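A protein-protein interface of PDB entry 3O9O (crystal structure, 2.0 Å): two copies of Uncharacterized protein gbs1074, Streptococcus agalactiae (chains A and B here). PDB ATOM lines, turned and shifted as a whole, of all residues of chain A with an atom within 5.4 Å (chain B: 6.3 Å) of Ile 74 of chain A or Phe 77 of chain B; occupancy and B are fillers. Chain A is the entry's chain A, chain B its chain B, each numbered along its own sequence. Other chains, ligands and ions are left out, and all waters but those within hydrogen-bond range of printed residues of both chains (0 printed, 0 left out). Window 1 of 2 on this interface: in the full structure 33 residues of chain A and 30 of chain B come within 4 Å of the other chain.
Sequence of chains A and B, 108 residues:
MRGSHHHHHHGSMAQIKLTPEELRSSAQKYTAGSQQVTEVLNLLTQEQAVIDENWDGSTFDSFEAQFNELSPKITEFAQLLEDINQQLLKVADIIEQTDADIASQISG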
ATOM      1  N   VAL A  37     -12.252 -16.779 -17.459  1.00  0.00           N
ATOM      2  CA  VAL A  37     -11.219 -17.521 -16.756  1.00  0.00           C
ATOM      3  C   VAL A  37     -11.811 -18.740 -16.049  1.00  0.00           C
ATOM      4  O   VAL A  37     -11.228 -19.818 -16.069  1.00  0.00           O
ATOM      5  CB  VAL A  37     -10.484 -16.631 -15.741  1.00  0.00           C
ATOM      6  CG1 VAL A  37      -9.755 -17.483 -14.710  1.00  0.00           C
ATOM      7  CG2 VAL A  37      -9.523 -15.708 -16.475  1.00  0.00           C
ATOM      8  N   VAL A  40     -12.703 -21.529 -18.647  1.00  0.00           N
ATOM      9  CA  VAL A  40     -11.505 -22.253 -19.062  1.00  0.00           C
ATOM     10  C   VAL A  40     -11.104 -23.240 -17.970  1.00  0.00           C
ATOM     11  O   VAL A  40     -10.884 -24.411 -18.249  1.00  0.00           O
ATOM     12  CB  VAL A  40     -10.323 -21.308 -19.365  1.00  0.00           C
ATOM     13  CG1 VAL A  40      -9.027 -22.118 -19.582  1.00  0.00           C
ATOM     14  CG2 VAL A  40     -10.628 -20.420 -20.590  1.00  0.00           C
ATOM     15  N   LEU A  41     -11.016 -22.773 -16.727  1.00  0.00           N
ATOM     16  CA  LEU A  41     -10.659 -23.651 -15.614  1.00  0.00           C
ATOM     17  C   LEU A  41     -11.602 -24.838 -15.555  1.00  0.00           C
ATOM     18  O   LEU A  41     -11.160 -25.972 -15.418  1.00  0.00           O
ATOM     19  CB  LEU A  41     -10.688 -22.905 -14.265  1.00  0.00           C
ATOM     20  CG  LEU A  41     -10.386 -23.754 -13.015  1.00  0.00           C
ATOM     21  CD1 LEU A  41      -8.946 -24.289 -13.036  1.00  0.00           C
ATOM     22  CD2 LEU A  41     -10.639 -22.969 -11.722  1.00  0.00           C
ATOM     23  N   PHE A  67      -1.185 -28.386 -12.612  1.00  0.00           N
ATOM     24  CA  PHE A  67      -2.552 -27.912 -12.794  1.00  0.00           C
ATOM     25  C   PHE A  67      -3.275 -27.844 -11.448  1.00  0.00           C
ATOM     26  O   PHE A  67      -3.885 -26.832 -11.123  1.00  0.00           O
ATOM     27  CB  PHE A  67      -3.299 -28.822 -13.775  1.00  0.00           C
ATOM     28  CG  PHE A  67      -4.623 -28.267 -14.256  1.00  0.00           C
ATOM     29  CD1 PHE A  67      -4.721 -27.643 -15.490  1.00  0.00           C
ATOM     30  CD2 PHE A  67      -5.771 -28.405 -13.489  1.00  0.00           C
ATOM     31  CE1 PHE A  67      -5.938 -27.147 -15.949  1.00  0.00           C
ATOM     32  CE2 PHE A  67      -6.999 -27.917 -13.941  1.00  0.00           C
ATOM     33  CZ  PHE A  67      -7.087 -27.291 -15.174  1.00  0.00           C
ATOM     34  N   LEU A  70      -2.132 -24.974  -9.209  1.00  0.00           N
ATOM     35  CA  LEU A  70      -2.519 -23.653  -9.705  1.00  0.00           C
ATOM     36  C   LEU A  70      -4.025 -23.399  -9.663  1.00  0.00           C
ATOM     37  O   LEU A  70      -4.462 -22.250  -9.540  1.00  0.00           O
ATOM     38  CB  LEU A  70      -2.025 -23.469 -11.137  1.00  0.00           C
ATOM     39  CG  LEU A  70      -0.534 -23.179 -11.271  1.00  0.00           C
ATOM     40  CD1 LEU A  70      -0.122 -23.205 -12.734  1.00  0.00           C
ATOM     41  CD2 LEU A  70      -0.201 -21.833 -10.626  1.00  0.00           C
ATOM     42  N   SER A  71      -4.812 -24.466  -9.768  1.00  0.00           N
ATOM     43  CA  SER A  71      -6.267 -24.352  -9.817  1.00  0.00           C
ATOM     44  C   SER A  71      -6.833 -23.388  -8.765  1.00  0.00           C
ATOM     45  O   SER A  71      -7.573 -22.473  -9.107  1.00  0.00           O
ATOM     46  CB  SER A  71      -6.915 -25.727  -9.664  1.00  0.00           C
ATOM     47  OG  SER A  71      -8.322 -25.603  -9.609  1.00  0.00           O
ATOM     48  N   PRO A  72      -6.486 -23.592  -7.482  1.00  0.00           N
ATOM     49  CA  PRO A  72      -7.000 -22.733  -6.405  1.00  0.00           C
ATOM     50  C   PRO A  72      -6.670 -21.255  -6.608  1.00  0.00           C
ATOM     51  O   PRO A  72      -7.477 -20.393  -6.253  1.00  0.00           O
ATOM     52  CB  PRO A  72      -6.286 -23.263  -5.156  1.00  0.00           C
ATOM     53  CG  PRO A  72      -5.842 -24.643  -5.511  1.00  0.00           C
ATOM     54  CD  PRO A  72      -5.565 -24.624  -6.976  1.00  0.00           C
ATOM     55  N   LYS A  73      -5.504 -20.966  -7.176  1.00  0.00           N
ATOM     56  CA  LYS A  73      -5.107 -19.587  -7.446  1.00  0.00           C
ATOM     57  C   LYS A  73      -5.896 -19.001  -8.617  1.00  0.00           C
ATOM     58  O   LYS A  73      -6.118 -17.791  -8.678  1.00  0.00           O
ATOM     59  CB  LYS A  73      -3.609 -19.504  -7.738  1.00  0.00           C
ATOM     60  CG  LYS A  73      -2.724 -20.182  -6.689  1.00  0.00           C
ATOM     61  CD  LYS A  73      -2.934 -19.616  -5.290  1.00  0.00           C
ATOM     62  CE  LYS A  73      -2.273 -18.260  -5.122  1.00  0.00           C
ATOM     63  NZ  LYS A  73      -2.496 -17.699  -3.758  1.00  0.00           N
ATOM     64  N   ILE A  74      -6.310 -19.851  -9.551  1.00  0.00           N
ATOM     65  CA  ILE A  74      -7.123 -19.395 -10.676  1.00  0.00           C
ATOM     66  C   ILE A  74      -8.506 -19.013 -10.158  1.00  0.00           C
ATOM     67  O   ILE A  74      -9.064 -17.981 -10.537  1.00  0.00           O
ATOM     68  CB  ILE A  74      -7.247 -20.461 -11.785  1.00  0.00           C
ATOM     69  CG1 ILE A  74      -5.860 -20.971 -12.203  1.00  0.00           C
ATOM     70  CG2 ILE A  74      -7.975 -19.891 -12.982  1.00  0.00           C
ATOM     71  CD1 ILE A  74      -4.878 -19.867 -12.602  1.00  0.00           C
ATOM     72  N   THR A  75      -9.038 -19.840  -9.267  1.00  0.00           N
ATOM     73  CA  THR A  75     -10.287 -19.530  -8.583  1.00  0.00           C
ATOM     74  C   THR A  75     -10.189 -18.223  -7.781  1.00  0.00           C
ATOM     75  O   THR A  75     -11.086 -17.378  -7.848  1.00  0.00           O
ATOM     76  CB  THR A  75     -10.696 -20.695  -7.665  1.00  0.00           C
ATOM     77  OG1 THR A  75     -10.962 -21.848  -8.470  1.00  0.00           O
ATOM     78  CG2 THR A  75     -11.938 -20.359  -6.874  1.00  0.00           C
ATOM     79  N   GLU A  76      -9.106 -18.043  -7.031  1.00  0.00           N
ATOM     80  CA  GLU A  76      -8.934 -16.802  -6.268  1.00  0.00           C
ATOM     81  C   GLU A  76      -8.919 -15.615  -7.209  1.00  0.00           C
ATOM     82  O   GLU A  76      -9.544 -14.588  -6.937  1.00  0.00           O
ATOM     83  CB  GLU A  76      -7.634 -16.806  -5.458  1.00  0.00           C
ATOM     84  CG  GLU A  76      -7.624 -17.783  -4.307  1.00  0.00           C
ATOM     85  CD  GLU A  76      -6.270 -17.858  -3.638  1.00  0.00           C
ATOM     86  OE1 GLU A  76      -5.576 -16.820  -3.596  1.00  0.00           O
ATOM     87  OE2 GLU A  76      -5.900 -18.954  -3.164  1.00  0.00           O
ATOM     88  N   PHE A  77      -8.210 -15.764  -8.325  1.00  0.00           N
ATOM     89  CA  PHE A  77      -8.093 -14.696  -9.317  1.00  0.00           C
ATOM     90  C   PHE A  77      -9.437 -14.317  -9.935  1.00  0.00           C
ATOM     91  O   PHE A  77      -9.741 -13.136 -10.090  1.00  0.00           O
ATOM     92  CB  PHE A  77      -7.108 -15.086 -10.416  1.00  0.00           C
ATOM     93  CG  PHE A  77      -6.831 -13.982 -11.402  1.00  0.00           C
ATOM     94  CD1 PHE A  77      -6.068 -12.886 -11.039  1.00  0.00           C
ATOM     95  CD2 PHE A  77      -7.320 -14.051 -12.692  1.00  0.00           C
ATOM     96  CE1 PHE A  77      -5.800 -11.877 -11.945  1.00  0.00           C
ATOM     97  CE2 PHE A  77      -7.056 -13.049 -13.601  1.00  0.00           C
ATOM     98  CZ  PHE A  77      -6.291 -11.956 -13.222  1.00  0.00           C
ATOM     99  N   ALA A  78     -10.249 -15.309 -10.286  1.00  0.00           N
ATOM    100  CA  ALA A  78     -11.576 -15.018 -10.827  1.00  0.00           C
ATOM    101  C   ALA A  78     -12.434 -14.309  -9.777  1.00  0.00           C
ATOM    102  O   ALA A  78     -13.225 -13.428 -10.100  1.00  0.00           O
ATOM    103  CB  ALA A  78     -12.265 -16.305 -11.308  1.00  0.00           C
ATOM    104  N   GLN A  79     -12.291 -14.695  -8.517  1.00  0.00           N
ATOM    105  CA  GLN A  79     -13.082 -14.060  -7.466  1.00  0.00           C
ATOM    106  C   GLN A  79     -12.647 -12.602  -7.273  1.00  0.00           C
ATOM    107  O   GLN A  79     -13.474 -11.725  -7.048  1.00  0.00           O
ATOM    108  CB  GLN A  79     -12.966 -14.839  -6.155  1.00  0.00           C
ATOM    109  CG  GLN A  79     -13.810 -14.260  -5.024  1.00  0.00           C
ATOM    110  CD  GLN A  79     -15.294 -14.220  -5.357  1.00  0.00           C
ATOM    111  OE1 GLN A  79     -15.895 -13.150  -5.483  1.00  0.00           O
ATOM    112  NE2 GLN A  79     -15.890 -15.389  -5.504  1.00  0.00           N
ATOM    113  N   SER B  34      -5.467 -21.525 -23.242  1.00  0.00           N
ATOM    114  CA  SER B  34      -4.275 -20.730 -22.944  1.00  0.00           C
ATOM    115  C   SER B  34      -4.384 -19.321 -23.528  1.00  0.00           C
ATOM    116  O   SER B  34      -3.999 -18.345 -22.891  1.00  0.00           O
ATOM    117  CB  SER B  34      -3.025 -21.411 -23.513  1.00  0.00           C
ATOM    118  OG  SER B  34      -1.868 -20.632 -23.271  1.00  0.00           O
ATOM    119  N   VAL B  37      -6.997 -17.118 -21.550  1.00  0.00           N
ATOM    120  CA  VAL B  37      -6.522 -16.698 -20.237  1.00  0.00           C
ATOM    121  C   VAL B  37      -5.528 -15.558 -20.397  1.00  0.00           C
ATOM    122  O   VAL B  37      -5.536 -14.597 -19.628  1.00  0.00           O
ATOM    123  CB  VAL B  37      -5.878 -17.858 -19.460  1.00  0.00           C
ATOM    124  CG1 VAL B  37      -5.151 -17.346 -18.225  1.00  0.00           C
ATOM    125  CG2 VAL B  37      -6.940 -18.872 -19.063  1.00  0.00           C
ATOM    126  N   LEU B  70      -1.208 -12.307  -7.727  1.00  0.00           N
ATOM    127  CA  LEU B  70      -1.831 -13.447  -8.389  1.00  0.00           C
ATOM    128  C   LEU B  70      -1.421 -13.552  -9.850  1.00  0.00           C
ATOM    129  O   LEU B  70      -1.456 -14.630 -10.435  1.00  0.00           O
ATOM    130  CB  LEU B  70      -3.352 -13.346  -8.299  1.00  0.00           C
ATOM    131  CG  LEU B  70      -3.962 -13.839  -6.990  1.00  0.00           C
ATOM    132  CD1 LEU B  70      -5.428 -13.449  -6.935  1.00  0.00           C
ATOM    133  CD2 LEU B  70      -3.793 -15.350  -6.842  1.00  0.00           C
ATOM    134  N   PRO B  72       1.362 -13.644 -11.552  1.00  0.00           N
ATOM    135  CA  PRO B  72       2.340 -14.666 -11.950  1.00  0.00           C
ATOM    136  C   PRO B  72       1.743 -16.071 -11.933  1.00  0.00           C
ATOM    137  O   PRO B  72       2.138 -16.911 -12.734  1.00  0.00           O
ATOM    138  CB  PRO B  72       3.439 -14.540 -10.890  1.00  0.00           C
ATOM    139  CG  PRO B  72       3.235 -13.192 -10.276  1.00  0.00           C
ATOM    140  CD  PRO B  72       1.769 -12.947 -10.323  1.00  0.00           C
ATOM    141  N   LYS B  73       0.809 -16.325 -11.026  1.00  0.00           N
ATOM    142  CA  LYS B  73       0.104 -17.590 -11.041  1.00  0.00           C
ATOM    143  C   LYS B  73      -0.647 -17.730 -12.365  1.00  0.00           C
ATOM    144  O   LYS B  73      -0.721 -18.818 -12.936  1.00  0.00           O
ATOM    145  CB  LYS B  73      -0.845 -17.697  -9.842  1.00  0.00           C
ATOM    146  CG  LYS B  73      -0.133 -17.823  -8.491  1.00  0.00           C
ATOM    147  CD  LYS B  73       1.200 -18.567  -8.623  1.00  0.00           C
ATOM    148  CE  LYS B  73       1.647 -19.201  -7.311  1.00  0.00           C
ATOM    149  NZ  LYS B  73       1.878 -18.215  -6.219  1.00  0.00           N
ATOM    150  N   ILE B  74      -1.173 -16.616 -12.868  1.00  0.00           N
ATOM    151  CA  ILE B  74      -2.004 -16.642 -14.068  1.00  0.00           C
ATOM    152  C   ILE B  74      -1.180 -16.854 -15.338  1.00  0.00           C
ATOM    153  O   ILE B  74      -1.615 -17.551 -16.256  1.00  0.00           O
ATOM    154  CB  ILE B  74      -2.842 -15.358 -14.207  1.00  0.00           C
ATOM    155  CG1 ILE B  74      -3.621 -15.088 -12.914  1.00  0.00           C
ATOM    156  CG2 ILE B  74      -3.791 -15.476 -15.390  1.00  0.00           C
ATOM    157  CD1 ILE B  74      -4.503 -16.260 -12.468  1.00  0.00           C
ATOM    158  N   THR B  75       0.007 -16.262 -15.404  1.00  0.00           N
ATOM    159  CA  THR B  75       0.876 -16.497 -16.555  1.00  0.00           C
ATOM    160  C   THR B  75       1.438 -17.920 -16.517  1.00  0.00           C
ATOM    161  O   THR B  75       1.535 -18.568 -17.552  1.00  0.00           O
ATOM    162  CB  THR B  75       2.035 -15.487 -16.651  1.00  0.00           C
ATOM    163  OG1 THR B  75       1.512 -14.165 -16.823  1.00  0.00           O
ATOM    164  CG2 THR B  75       2.906 -15.820 -17.846  1.00  0.00           C
ATOM    165  N   GLU B  76       1.793 -18.396 -15.325  1.00  0.00           N
ATOM    166  CA  GLU B  76       2.211 -19.785 -15.130  1.00  0.00           C
ATOM    167  C   GLU B  76       1.146 -20.736 -15.686  1.00  0.00           C
ATOM    168  O   GLU B  76       1.462 -21.754 -16.303  1.00  0.00           O
ATOM    169  CB  GLU B  76       2.448 -20.078 -13.635  1.00  0.00           C
ATOM    170  CG  GLU B  76       3.018 -21.487 -13.338  1.00  0.00           C
ATOM    171  CD  GLU B  76       3.160 -21.797 -11.841  1.00  0.00           C
ATOM    172  OE1 GLU B  76       3.243 -20.853 -11.027  1.00  0.00           O
ATOM    173  OE2 GLU B  76       3.194 -22.992 -11.473  1.00  0.00           O
ATOM    174  N   PHE B  77      -0.118 -20.391 -15.473  1.00  0.00           N
ATOM    175  CA  PHE B  77      -1.234 -21.235 -15.889  1.00  0.00           C
ATOM    176  C   PHE B  77      -1.390 -21.258 -17.410  1.00  0.00           C
ATOM    177  O   PHE B  77      -1.536 -22.323 -18.017  1.00  0.00           O
ATOM    178  CB  PHE B  77      -2.525 -20.739 -15.237  1.00  0.00           C
ATOM    179  CG  PHE B  77      -3.695 -21.670 -15.406  1.00  0.00           C
ATOM    180  CD1 PHE B  77      -3.657 -22.955 -14.885  1.00  0.00           C
ATOM    181  CD2 PHE B  77      -4.843 -21.250 -16.057  1.00  0.00           C
ATOM    182  CE1 PHE B  77      -4.742 -23.805 -15.013  1.00  0.00           C
ATOM    183  CE2 PHE B  77      -5.933 -22.100 -16.200  1.00  0.00           C
ATOM    184  CZ  PHE B  77      -5.881 -23.380 -15.673  1.00  0.00           C
ATOM    185  N   ALA B  78      -1.355 -20.084 -18.026  1.00  0.00           N
ATOM    186  CA  ALA B  78      -1.485 -19.995 -19.470  1.00  0.00           C
ATOM    187  C   ALA B  78      -0.366 -20.779 -20.154  1.00  0.00           C
ATOM    188  O   ALA B  78      -0.586 -21.415 -21.182  1.00  0.00           O
ATOM    189  CB  ALA B  78      -1.461 -18.555 -19.920  1.00  0.00           C
ATOM    190  N   GLN B  79       0.835 -20.733 -19.593  1.00  0.00           N
ATOM    191  CA  GLN B  79       1.962 -21.429 -20.214  1.00  0.00           C
ATOM    192  C   GLN B  79       1.873 -22.938 -19.974  1.00  0.00           C
ATOM    193  O   GLN B  79       2.322 -23.725 -20.803  1.00  0.00           O
ATOM    194  CB  GLN B  79       3.299 -20.871 -19.715  1.00  0.00           C
ATOM    195  CG  GLN B  79       4.522 -21.444 -20.442  1.00  0.00           C
ATOM    196  CD  GLN B  79       4.377 -21.444 -21.959  1.00  0.00           C
ATOM    197  OE1 GLN B  79       4.505 -22.488 -22.608  1.00  0.00           O
ATOM    198  NE2 GLN B  79       4.108 -20.273 -22.532  1.00  0.00           N
ATOM    199  N   LEU B  80       1.289 -23.338 -18.848  1.00  0.00           N
ATOM    200  CA  LEU B  80       1.069 -24.751 -18.575  1.00  0.00           C
ATOM    201  C   LEU B  80       0.118 -25.303 -19.619  1.00  0.00           C
ATOM    202  O   LEU B  80       0.359 -26.368 -20.181  1.00  0.00           O
ATOM    203  CB  LEU B  80       0.496 -24.959 -17.171  1.00  0.00           C
ATOM    204  CG  LEU B  80       0.025 -26.371 -16.805  1.00  0.00           C
ATOM    205  CD1 LEU B  80       1.145 -27.403 -17.008  1.00  0.00           C
ATOM    206  CD2 LEU B  80      -0.493 -26.413 -15.363  1.00  0.00           C
ATOM    207  N   LEU B  81      -0.953 -24.562 -19.898  1.00  0.00           N
ATOM    208  CA  LEU B  81      -1.972 -25.024 -20.834  1.00  0.00           C
ATOM    209  C   LEU B  81      -1.389 -25.181 -22.233  1.00  0.00           C
ATOM    210  O   LEU B  81      -1.711 -26.130 -22.949  1.00  0.00           O
ATOM    211  CB  LEU B  81      -3.176 -24.071 -20.873  1.00  0.00           C
ATOM    212  CG  LEU B  81      -3.924 -23.840 -19.554  1.00  0.00           C
ATOM    213  CD1 LEU B  81      -5.223 -23.065 -19.792  1.00  0.00           C
ATOM    214  CD2 LEU B  81      -4.214 -25.155 -18.852  1.00  0.00           C
ATOM    215  N   GLU B  82      -0.535 -24.244 -22.621  1.00  0.00           N
ATOM    216  CA  GLU B  82       0.094 -24.300 -23.933  1.00  0.00           C
ATOM    217  C   GLU B  82       1.085 -25.459 -24.004  1.00  0.00           C
ATOM    218  O   GLU B  82       1.233 -26.098 -25.046  1.00  0.00           O
ATOM    219  CB  GLU B  82       0.812 -22.984 -24.237  1.00  0.00           C
ATOM    220  CG  GLU B  82       1.421 -22.930 -25.625  1.00  0.00           C
ATOM    221  CD  GLU B  82       0.416 -23.268 -26.711  1.00  0.00           C
ATOM    222  OE1 GLU B  82      -0.788 -23.010 -26.510  1.00  0.00           O
ATOM    223  OE2 GLU B  82       0.828 -23.792 -27.766  1.00  0.00           O
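NZ of Lys 73 of chain A lies within salt-bridge range of OE1 of Glu 76 of chain A (3.2 Å).
Val 40 of chain A touches Val 37 of chain B. Phe 77 of chain B touches Phe 67 of chain A (CE1 to CE1, 3.7 Å). Phe 67 of chain A touches Leu 81 of chain B (CE1 to CD2, 3.9 Å). CD2 of Leu 70 of chain A touches O of Lys 73 of chain B (3.8 Å). Leu 70 of chain A touches Glu 76 of chain B (CD1 to OE2, 3.6 Å). Phe 77 of chain B touches Leu 70 of chain A. CD2 of Leu 70 of chain B touches CE of Lys 73 of chain A, at 3.7 Å. Lys 73 of chain A touches Lys 73 of chain B (CB to CB, 3.9 Å). Ile 74 of chain A touches Ile 74 of chain B (CD1 to CD1, 3.6 Å). Ile 74 of chain B touches Phe 77 of chain A.
Of the printed residues of chain B, Phe 67 of chain A touches Phe 77 (3.7 Å), Leu 80 (3.5 Å) and Leu 81 (3.9 Å). Of the printed residues of chain B, Lys 73 of chain A touches Leu 70 and Lys 73. Of chain B, only Ile 74 and Phe 77 come within 4 Å of Ile 74 of chain A. Of the printed residues of chain B, Glu 76 of chain A touches Leu 70 (3.98 Å). Of the printed residues of chain A, Leu 70 of chain B touches Lys 73, Glu 76 and Phe 77. Phe 77 of chain B touches just these residues of chain A: Phe 67, Leu 70 and Ile 74. The nearest residue of chain A that does not touch Phe 77 of chain B is Leu 41 of chain A (4.1 Å). The nearest printed residue of chain B that does not touch Phe 67 of chain A is Glu 76 of chain B (7.0 Å).
Of the 14 printed residues of chain A, 7 touch a printed residue of chain B. Hydrophobic or aromatic side chains of chain A that line the printed part of chain B: Val 40, Phe 67, Leu 70, Ile 74 and Phe 77. Along chain A the printed residues that touch a printed residue of chain B span positions 40 to 77. Of the 14 printed residues of chain B, 8 touch a printed residue of chain A. Printed residues of chain B that touch a printed residue of chain A: Val 37, Leu 70, Lys 73, Ile 74, Glu 76, Phe 77, Leu 80 and Leu 81. Among the printed residues, no Asp or Glu carboxylate lies within 4 Å of a Lys or Arg side-chain nitrogen of the other chain.
Leu 70 of chain A touches Glu 76 of chain B, and with the chains exchanged Glu 76 of chain A touches Leu 70 of chain B. Leu 70 of chain A touches Phe 77 of chain B, and with the chains exchanged Phe 77 of chain A touches Leu 70 of chain B. Ile 74 of chain A touches its own counterpart, Ile 74 of chain B. Ile 74 of chain A touches Phe 77 of chain B, and with the chains exchanged Phe 77 of chain A touches Ile 74 of chain B. 10 positions are printed for both chains.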
